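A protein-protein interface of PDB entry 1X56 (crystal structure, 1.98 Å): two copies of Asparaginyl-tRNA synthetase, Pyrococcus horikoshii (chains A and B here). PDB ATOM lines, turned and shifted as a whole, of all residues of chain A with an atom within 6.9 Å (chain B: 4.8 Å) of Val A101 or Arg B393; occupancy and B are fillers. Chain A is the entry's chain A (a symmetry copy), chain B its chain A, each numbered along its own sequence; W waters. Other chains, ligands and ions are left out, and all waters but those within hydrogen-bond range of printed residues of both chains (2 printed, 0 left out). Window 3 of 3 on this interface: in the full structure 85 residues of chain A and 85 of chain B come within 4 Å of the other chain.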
ATOM      1  N   VAL A  25      15.281  10.147   6.441  1.00  0.00           N
ATOM      2  CA  VAL A  25      15.237  11.604   6.170  1.00  0.00           C
ATOM      3  C   VAL A  25      16.427  12.342   6.810  1.00  0.00           C
ATOM      4  O   VAL A  25      16.673  12.286   8.034  1.00  0.00           O
ATOM      5  CB  VAL A  25      13.897  12.246   6.543  1.00  0.00           C
ATOM      6  CG1 VAL A  25      13.930  13.783   6.234  1.00  0.00           C
ATOM      7  CG2 VAL A  25      12.740  11.550   5.769  1.00  0.00           C
ATOM      8  N   LYS A  65       5.302  16.009   7.912  1.00  0.00           N
ATOM      9  CA  LYS A  65       5.599  15.635   9.276  1.00  0.00           C
ATOM     10  C   LYS A  65       6.925  14.864   9.419  1.00  0.00           C
ATOM     11  O   LYS A  65       7.283  14.455  10.523  1.00  0.00           O
ATOM     12  CB  LYS A  65       4.486  14.731   9.792  1.00  0.00           C
ATOM     13  CG  LYS A  65       3.121  15.376   9.805  1.00  0.00           C
ATOM     14  CD  LYS A  65       2.160  14.439  10.572  1.00  0.00           C
ATOM     15  CE  LYS A  65       0.733  14.966  10.572  1.00  0.00           C
ATOM     16  NZ  LYS A  65       0.754  16.447  10.430  1.00  0.00           N
ATOM     17  N   LEU A  66       7.633  14.624   8.325  1.00  0.00           N
ATOM     18  CA  LEU A  66       8.834  13.789   8.404  1.00  0.00           C
ATOM     19  C   LEU A  66      10.072  14.544   8.840  1.00  0.00           C
ATOM     20  O   LEU A  66      10.652  15.301   8.058  1.00  0.00           O
ATOM     21  CB  LEU A  66       9.108  13.064   7.085  1.00  0.00           C
ATOM     22  CG  LEU A  66       7.989  12.136   6.620  1.00  0.00           C
ATOM     23  CD1 LEU A  66       8.292  11.652   5.159  1.00  0.00           C
ATOM     24  CD2 LEU A  66       7.664  10.997   7.608  1.00  0.00           C
ATOM     25  N   GLY A  67      10.458  14.335  10.093  1.00  0.00           N
ATOM     26  CA  GLY A  67      11.647  14.981  10.624  1.00  0.00           C
ATOM     27  C   GLY A  67      12.848  14.098  10.314  1.00  0.00           C
ATOM     28  O   GLY A  67      12.713  13.032   9.688  1.00  0.00           O
ATOM     29  N   ARG A  68      14.000  14.555  10.787  1.00  0.00           N
ATOM     30  CA  ARG A  68      15.264  13.872  10.666  1.00  0.00           C
ATOM     31  C   ARG A  68      15.217  12.461  11.230  1.00  0.00           C
ATOM     32  O   ARG A  68      14.741  12.241  12.356  1.00  0.00           O
ATOM     33  CB  ARG A  68      16.316  14.665  11.430  1.00  0.00           C
ATOM     34  CG  ARG A  68      16.674  15.978  10.778  1.00  0.00           C
ATOM     35  CD  ARG A  68      17.989  16.540  11.309  1.00  0.00           C
ATOM     36  NE  ARG A  68      17.948  16.586  12.772  1.00  0.00           N
ATOM     37  CZ  ARG A  68      18.848  16.049  13.590  1.00  0.00           C
ATOM     38  NH1 ARG A  68      19.937  15.447  13.135  1.00  0.00           N
ATOM     39  NH2 ARG A  68      18.664  16.166  14.881  1.00  0.00           N
ATOM     40  N   GLU A  69      15.714  11.518  10.419  1.00  0.00           N
ATOM     41  CA  GLU A  69      15.779  10.088  10.765  1.00  0.00           C
ATOM     42  C   GLU A  69      14.467   9.320  10.587  1.00  0.00           C
ATOM     43  O   GLU A  69      14.392   8.103  10.892  1.00  0.00           O
ATOM     44  CB  GLU A  69      16.438   9.851  12.153  1.00  0.00           C
ATOM     45  CG  GLU A  69      17.911  10.266  12.209  1.00  0.00           C
ATOM     46  CD  GLU A  69      18.747   9.589  11.136  1.00  0.00           C
ATOM     47  OE1 GLU A  69      18.615   8.335  10.975  1.00  0.00           O
ATOM     48  OE2 GLU A  69      19.526  10.287  10.430  1.00  0.00           O
ATOM     49  N   SER A  70      13.438   9.985  10.034  1.00  0.00           N
ATOM     50  CA  SER A  70      12.252   9.226   9.563  1.00  0.00           C
ATOM     51  C   SER A  70      12.689   8.168   8.563  1.00  0.00           C
ATOM     52  O   SER A  70      13.458   8.478   7.643  1.00  0.00           O
ATOM     53  CB  SER A  70      11.196  10.145   8.914  1.00  0.00           C
ATOM     54  OG  SER A  70      10.820  11.195   9.819  1.00  0.00           O
ATOM     55  N   SER A  71      12.220   6.923   8.739  1.00  0.00           N
ATOM     56  CA  SER A  71      12.560   5.853   7.775  1.00  0.00           C
ATOM     57  C   SER A  71      11.507   5.777   6.704  1.00  0.00           C
ATOM     58  O   SER A  71      10.300   5.743   7.002  1.00  0.00           O
ATOM     59  CB  SER A  71      12.746   4.509   8.471  1.00  0.00           C
ATOM     60  OG  SER A  71      11.676   4.226   9.378  1.00  0.00           O
ATOM     61  N   VAL A  97       5.926   5.610   4.421  1.00  0.00           N
ATOM     62  CA  VAL A  97       6.531   6.056   5.664  1.00  0.00           C
ATOM     63  C   VAL A  97       6.616   4.853   6.586  1.00  0.00           C
ATOM     64  O   VAL A  97       5.579   4.308   7.015  1.00  0.00           O
ATOM     65  CB  VAL A  97       5.726   7.192   6.348  1.00  0.00           C
ATOM     66  CG1 VAL A  97       6.346   7.539   7.736  1.00  0.00           C
ATOM     67  CG2 VAL A  97       5.640   8.463   5.452  1.00  0.00           C
ATOM     68  N   GLN A  99       8.568   4.809   9.616  1.00  0.00           N
ATOM     69  CA  GLN A  99       8.434   5.425  10.915  1.00  0.00           C
ATOM     70  C   GLN A  99       8.801   6.906  10.858  1.00  0.00           C
ATOM     71  O   GLN A  99       9.938   7.245  10.573  1.00  0.00           O
ATOM     72  CB  GLN A  99       9.292   4.704  11.944  1.00  0.00           C
ATOM     73  CG  GLN A  99       9.064   5.252  13.339  1.00  0.00           C
ATOM     74  CD  GLN A  99       9.855   4.540  14.379  1.00  0.00           C
ATOM     75  OE1 GLN A  99      11.086   4.466  14.319  1.00  0.00           O
ATOM     76  NE2 GLN A  99       9.155   4.050  15.389  1.00  0.00           N
ATOM     77  N   ALA A 100       7.819   7.789  11.088  1.00  0.00           N
ATOM     78  CA  ALA A 100       8.058   9.235  11.161  1.00  0.00           C
ATOM     79  C   ALA A 100       8.756   9.554  12.469  1.00  0.00           C
ATOM     80  O   ALA A 100       8.415   9.037  13.495  1.00  0.00           O
ATOM     81  CB  ALA A 100       6.714  10.009  11.086  1.00  0.00           C
ATOM     82  N   VAL A 101       9.749  10.415  12.425  1.00  0.00           N
ATOM     83  CA  VAL A 101      10.474  10.815  13.608  1.00  0.00           C
ATOM     84  C   VAL A 101      10.496  12.343  13.600  1.00  0.00           C
ATOM     85  O   VAL A 101      10.644  12.948  12.552  1.00  0.00           O
ATOM     86  CB  VAL A 101      11.916  10.264  13.565  1.00  0.00           C
ATOM     87  CG1 VAL A 101      12.698  10.741  14.746  1.00  0.00           C
ATOM     88  CG2 VAL A 101      11.898   8.719  13.505  1.00  0.00           C
ATOM     89  N   SER A 102      10.397  12.972  14.758  1.00  0.00           N
ATOM     90  CA  SER A 102      10.501  14.447  14.782  1.00  0.00           C
ATOM     91  C   SER A 102      11.472  14.909  15.860  1.00  0.00           C
ATOM     92  O   SER A 102      11.847  16.071  15.892  1.00  0.00           O
ATOM     93  CB  SER A 102       9.135  15.056  15.004  1.00  0.00           C
ATOM     94  OG  SER A 102       8.635  14.603  16.248  1.00  0.00           O
ATOM     95  N   GLU A 103      11.923  13.993  16.713  1.00  0.00           N
ATOM     96  CA  GLU A 103      12.787  14.377  17.838  1.00  0.00           C
ATOM     97  C   GLU A 103      14.077  13.560  18.025  1.00  0.00           C
ATOM     98  O   GLU A 103      14.418  13.160  19.141  1.00  0.00           O
ATOM     99  CB  GLU A 103      11.978  14.337  19.119  1.00  0.00           C
ATOM    100  CG  GLU A 103      10.824  15.317  19.099  1.00  0.00           C
ATOM    101  CD  GLU A 103      10.207  15.410  20.461  1.00  0.00           C
ATOM    102  OE1 GLU A 103      10.471  16.434  21.146  1.00  0.00           O
ATOM    103  OE2 GLU A 103       9.509  14.434  20.847  1.00  0.00           O
ATOM    104  N   PHE A 104      14.812  13.357  16.942  1.00  0.00           N
ATOM    105  CA  PHE A 104      16.088  12.671  17.029  1.00  0.00           C
ATOM    106  C   PHE A 104      17.002  13.397  18.034  1.00  0.00           C
ATOM    107  O   PHE A 104      17.191  14.583  17.872  1.00  0.00           O
ATOM    108  CB  PHE A 104      16.725  12.618  15.632  1.00  0.00           C
ATOM    109  CG  PHE A 104      17.863  11.644  15.525  1.00  0.00           C
ATOM    110  CD1 PHE A 104      17.659  10.276  15.799  1.00  0.00           C
ATOM    111  CD2 PHE A 104      19.143  12.084  15.163  1.00  0.00           C
ATOM    112  CE1 PHE A 104      18.732   9.357  15.686  1.00  0.00           C
ATOM    113  CE2 PHE A 104      20.211  11.169  15.078  1.00  0.00           C
ATOM    114  CZ  PHE A 104      19.983   9.809  15.342  1.00  0.00           C
ATOM    115  N   PRO A 105      17.560  12.710  19.041  1.00  0.00           N
ATOM    116  CA  PRO A 105      18.334  13.359  20.096  1.00  0.00           C
ATOM    117  C   PRO A 105      19.707  13.932  19.707  1.00  0.00           C
ATOM    118  O   PRO A 105      20.294  14.671  20.498  1.00  0.00           O
ATOM    119  CB  PRO A 105      18.586  12.223  21.100  1.00  0.00           C
ATOM    120  CG  PRO A 105      17.741  11.142  20.728  1.00  0.00           C
ATOM    121  CD  PRO A 105      17.489  11.257  19.260  1.00  0.00           C
ATOM    122  N   ARG A 127      25.399   6.571  13.559  1.00  0.00           N
ATOM    123  CA  ARG A 127      24.761   6.646  12.233  1.00  0.00           C
ATOM    124  C   ARG A 127      25.043   7.950  11.470  1.00  0.00           C
ATOM    125  O   ARG A 127      24.864   7.995  10.239  1.00  0.00           O
ATOM    126  CB  ARG A 127      23.243   6.324  12.257  1.00  0.00           C
ATOM    127  CG  ARG A 127      22.392   7.417  12.782  1.00  0.00           C
ATOM    128  CD  ARG A 127      20.939   7.113  12.746  1.00  0.00           C
ATOM    129  NE  ARG A 127      20.542   6.046  13.650  1.00  0.00           N
ATOM    130  CZ  ARG A 127      19.277   5.715  13.876  1.00  0.00           C
ATOM    131  NH1 ARG A 127      18.266   6.360  13.245  1.00  0.00           N
ATOM    132  NH2 ARG A 127      19.001   4.718  14.720  1.00  0.00           N
ATOM    133  N   TYR B 368       8.358  -1.202  18.226  1.00  0.00           N
ATOM    134  CA  TYR B 368       8.648  -0.773  19.610  1.00  0.00           C
ATOM    135  C   TYR B 368       7.793  -1.458  20.706  1.00  0.00           C
ATOM    136  O   TYR B 368       8.344  -1.986  21.669  1.00  0.00           O
ATOM    137  CB  TYR B 368       8.537   0.762  19.755  1.00  0.00           C
ATOM    138  CG  TYR B 368       8.893   1.268  21.136  1.00  0.00           C
ATOM    139  CD1 TYR B 368       7.968   1.213  22.198  1.00  0.00           C
ATOM    140  CD2 TYR B 368      10.152   1.800  21.385  1.00  0.00           C
ATOM    141  CE1 TYR B 368       8.310   1.685  23.473  1.00  0.00           C
ATOM    142  CE2 TYR B 368      10.501   2.277  22.623  1.00  0.00           C
ATOM    143  CZ  TYR B 368       9.574   2.211  23.663  1.00  0.00           C
ATOM    144  OH  TYR B 368       9.958   2.683  24.870  1.00  0.00           O
ATOM    145  N   LEU B 389      15.867  -0.360  22.534  1.00  0.00           N
ATOM    146  CA  LEU B 389      14.519   0.118  22.220  1.00  0.00           C
ATOM    147  C   LEU B 389      14.545   1.406  21.420  1.00  0.00           C
ATOM    148  O   LEU B 389      13.692   1.616  20.582  1.00  0.00           O
ATOM    149  CB  LEU B 389      13.680   0.295  23.525  1.00  0.00           C
ATOM    150  CG  LEU B 389      13.118  -1.012  24.142  1.00  0.00           C
ATOM    151  CD1 LEU B 389      12.872  -0.837  25.643  1.00  0.00           C
ATOM    152  CD2 LEU B 389      11.836  -1.523  23.420  1.00  0.00           C
ATOM    153  N   ASP B 390      15.540   2.256  21.655  1.00  0.00           N
ATOM    154  CA  ASP B 390      15.732   3.474  20.805  1.00  0.00           C
ATOM    155  C   ASP B 390      15.742   3.174  19.312  1.00  0.00           C
ATOM    156  O   ASP B 390      15.301   3.990  18.490  1.00  0.00           O
ATOM    157  CB  ASP B 390      17.029   4.207  21.158  1.00  0.00           C
ATOM    158  CG  ASP B 390      16.889   5.093  22.365  1.00  0.00           C
ATOM    159  OD1 ASP B 390      15.725   5.377  22.783  1.00  0.00           O
ATOM    160  OD2 ASP B 390      17.889   5.548  22.946  1.00  0.00           O
ATOM    161  N   LEU B 391      16.295   2.015  18.948  1.00  0.00           N
ATOM    162  CA  LEU B 391      16.399   1.631  17.535  1.00  0.00           C
ATOM    163  C   LEU B 391      15.024   1.371  16.918  1.00  0.00           C
ATOM    164  O   LEU B 391      14.923   1.282  15.706  1.00  0.00           O
ATOM    165  CB  LEU B 391      17.354   0.425  17.330  1.00  0.00           C
ATOM    166  CG  LEU B 391      18.761   0.526  17.950  1.00  0.00           C
ATOM    167  CD1 LEU B 391      19.458  -0.830  17.714  1.00  0.00           C
ATOM    168  CD2 LEU B 391      19.576   1.758  17.371  1.00  0.00           C
ATOM    169  N   ARG B 392      13.981   1.194  17.740  1.00  0.00           N
ATOM    170  CA  ARG B 392      12.616   1.024  17.237  1.00  0.00           C
ATOM    171  C   ARG B 392      11.839   2.351  17.366  1.00  0.00           C
ATOM    172  O   ARG B 392      10.620   2.392  17.105  1.00  0.00           O
ATOM    173  CB  ARG B 392      11.876  -0.058  18.043  1.00  0.00           C
ATOM    174  CG  ARG B 392      12.299  -1.519  17.746  1.00  0.00           C
ATOM    175  CD  ARG B 392      13.775  -1.862  18.075  1.00  0.00           C
ATOM    176  NE  ARG B 392      14.082  -3.215  17.613  1.00  0.00           N
ATOM    177  CZ  ARG B 392      15.266  -3.794  17.735  1.00  0.00           C
ATOM    178  NH1 ARG B 392      16.275  -3.133  18.347  1.00  0.00           N
ATOM    179  NH2 ARG B 392      15.436  -5.041  17.248  1.00  0.00           N
ATOM    180  N   ARG B 393      12.550   3.403  17.783  1.00  0.00           N
ATOM    181  CA  ARG B 393      11.939   4.719  18.082  1.00  0.00           C
ATOM    182  C   ARG B 393      12.385   5.751  17.014  1.00  0.00           C
ATOM    183  O   ARG B 393      11.633   6.642  16.613  1.00  0.00           O
ATOM    184  CB  ARG B 393      12.356   5.141  19.504  1.00  0.00           C
ATOM    185  CG  ARG B 393      11.862   6.525  19.990  1.00  0.00           C
ATOM    186  CD  ARG B 393      12.309   6.871  21.411  1.00  0.00           C
ATOM    187  NE  ARG B 393      11.672   6.025  22.418  1.00  0.00           N
ATOM    188  CZ  ARG B 393      10.487   6.343  22.965  1.00  0.00           C
ATOM    189  NH1 ARG B 393       9.920   5.556  23.882  1.00  0.00           N
ATOM    190  NH2 ARG B 393       9.859   7.467  22.586  1.00  0.00           N
ATOM    191  N   TYR B 394      13.630   5.633  16.553  1.00  0.00           N
ATOM    192  CA  TYR B 394      14.186   6.658  15.692  1.00  0.00           C
ATOM    193  C   TYR B 394      14.381   6.190  14.246  1.00  0.00           C
ATOM    194  O   TYR B 394      15.502   6.249  13.717  1.00  0.00           O
ATOM    195  CB  TYR B 394      15.478   7.220  16.314  1.00  0.00           C
ATOM    196  CG  TYR B 394      15.249   7.827  17.699  1.00  0.00           C
ATOM    197  CD1 TYR B 394      14.459   8.980  17.850  1.00  0.00           C
ATOM    198  CD2 TYR B 394      15.790   7.242  18.853  1.00  0.00           C
ATOM    199  CE1 TYR B 394      14.211   9.534  19.117  1.00  0.00           C
ATOM    200  CE2 TYR B 394      15.568   7.795  20.133  1.00  0.00           C
ATOM    201  CZ  TYR B 394      14.774   8.938  20.236  1.00  0.00           C
ATOM    202  OH  TYR B 394      14.538   9.498  21.454  1.00  0.00           O
ATOM    203  N   GLY B 395      13.305   5.770  13.577  1.00  0.00           N
ATOM    204  CA  GLY B 395      13.423   5.386  12.179  1.00  0.00           C
ATOM    205  C   GLY B 395      13.725   3.894  12.063  1.00  0.00           C
ATOM    206  O   GLY B 395      14.580   3.469  11.261  1.00  0.00           O
HETATM  207  O   HOH W   1      16.307   3.669  14.797  1.00  0.00           O
HETATM  208  O   HOH W   2       8.427   0.963  16.283  1.00  0.00           O
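The side-chain hydroxyl (OH) of Tyr B368 sits at hydrogen-bond distance from the guanidinium group (NH1) of Arg B393. O of Val A25 is in hydrogen-bond range of N of Glu A69 (2.7 Å). The backbone NH of Gly A67 is in hydrogen-bond range of the backbone carbonyl oxygen of Val A101 (2.8 Å). OE1 of Glu A69 lies within salt-bridge range of NH1 of Arg A127 (3.0 Å). OG of Ser A70 sits at hydrogen-bond distance from N of Val A101 (2.9 Å). The backbone carbonyl oxygen (O) of Gln A99 sits at hydrogen-bond distance from the backbone NH (N) of Ser A71, at 2.9 Å.
Among the printed residues, pairs that only touch across the chains: Glu A69 with Tyr B394, Glu A69 with Gly B395, Ser A71 with Gly B395, Gln A99 with Tyr B394, Val A101 with Arg B393, Val A101 with Tyr B394, Val A101 with Gly B395, Glu A103 with Tyr B394, Phe A104 with Tyr B394 and Pro A105 with Tyr B394.
Val A101 touches just these residues of chain B: Arg B393, Tyr B394 and Gly B395. Arg B393 touches just these residues of chain A: Gln A99 and Val A101. Of the printed residues of chain A, Gly B395 touches Glu A69, Ser A71, Gln A99 and Val A101. Printed residues of chain B within 4 Å of Phe A104: Tyr B394 (3.8 Å). Printed residues of chain A within 4 Å of Arg B392: Gln A99. Lys A65 touches none of the printed residues of chain B. Ser A102 touches none of the printed residues of chain B. The nearest printed residue of chain B that does not touch Val A101 is Arg B392 (7.4 Å). The nearest residue of chain A that does not touch Arg B393 is Ala A100 (5.1 Å).
O of Arg B392 is in hydrogen-bond range of NE2 of Gln A99 (2.8 Å). The backbone carbonyl oxygen (O) of Arg B393 lies close to the side-chain amide oxygen (OE1) of Gln A99 (3.2 Å). The backbone carbonyl oxygen (O) of Tyr B394 lies within hydrogen-bond range of the guanidinium group (NH1) of Arg A127 (2.8 Å). The backbone NH (N) of Gly B395 lies within hydrogen-bond range of the side-chain amide oxygen (OE1) of Gln A99.
No position is printed for both chains.
Water W2 lies within hydrogen-bond range of O of Arg B392, N of Tyr B368 and NE2 of Gln A99. Water W1 lies within hydrogen-bond range of the guanidinium group (NH2) of Arg A127, the backbone carbonyl oxygen (O) of Leu B391 and the backbone carbonyl oxygen (O) of Tyr B394.
Hydrophobic or aromatic side chains of chain A within 4 Å of the printed part of chain B: Val A101, Phe A104 and Pro A105. Printed residues of chain B that touch a printed residue of chain A: Arg B392, Arg B393, Tyr B394 and Gly B395. Hydrophobic or aromatic side chains of chain B within 4 Å of the printed part of chain A: Tyr B394. Among the printed residues, 14 pairs touch across the chains.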
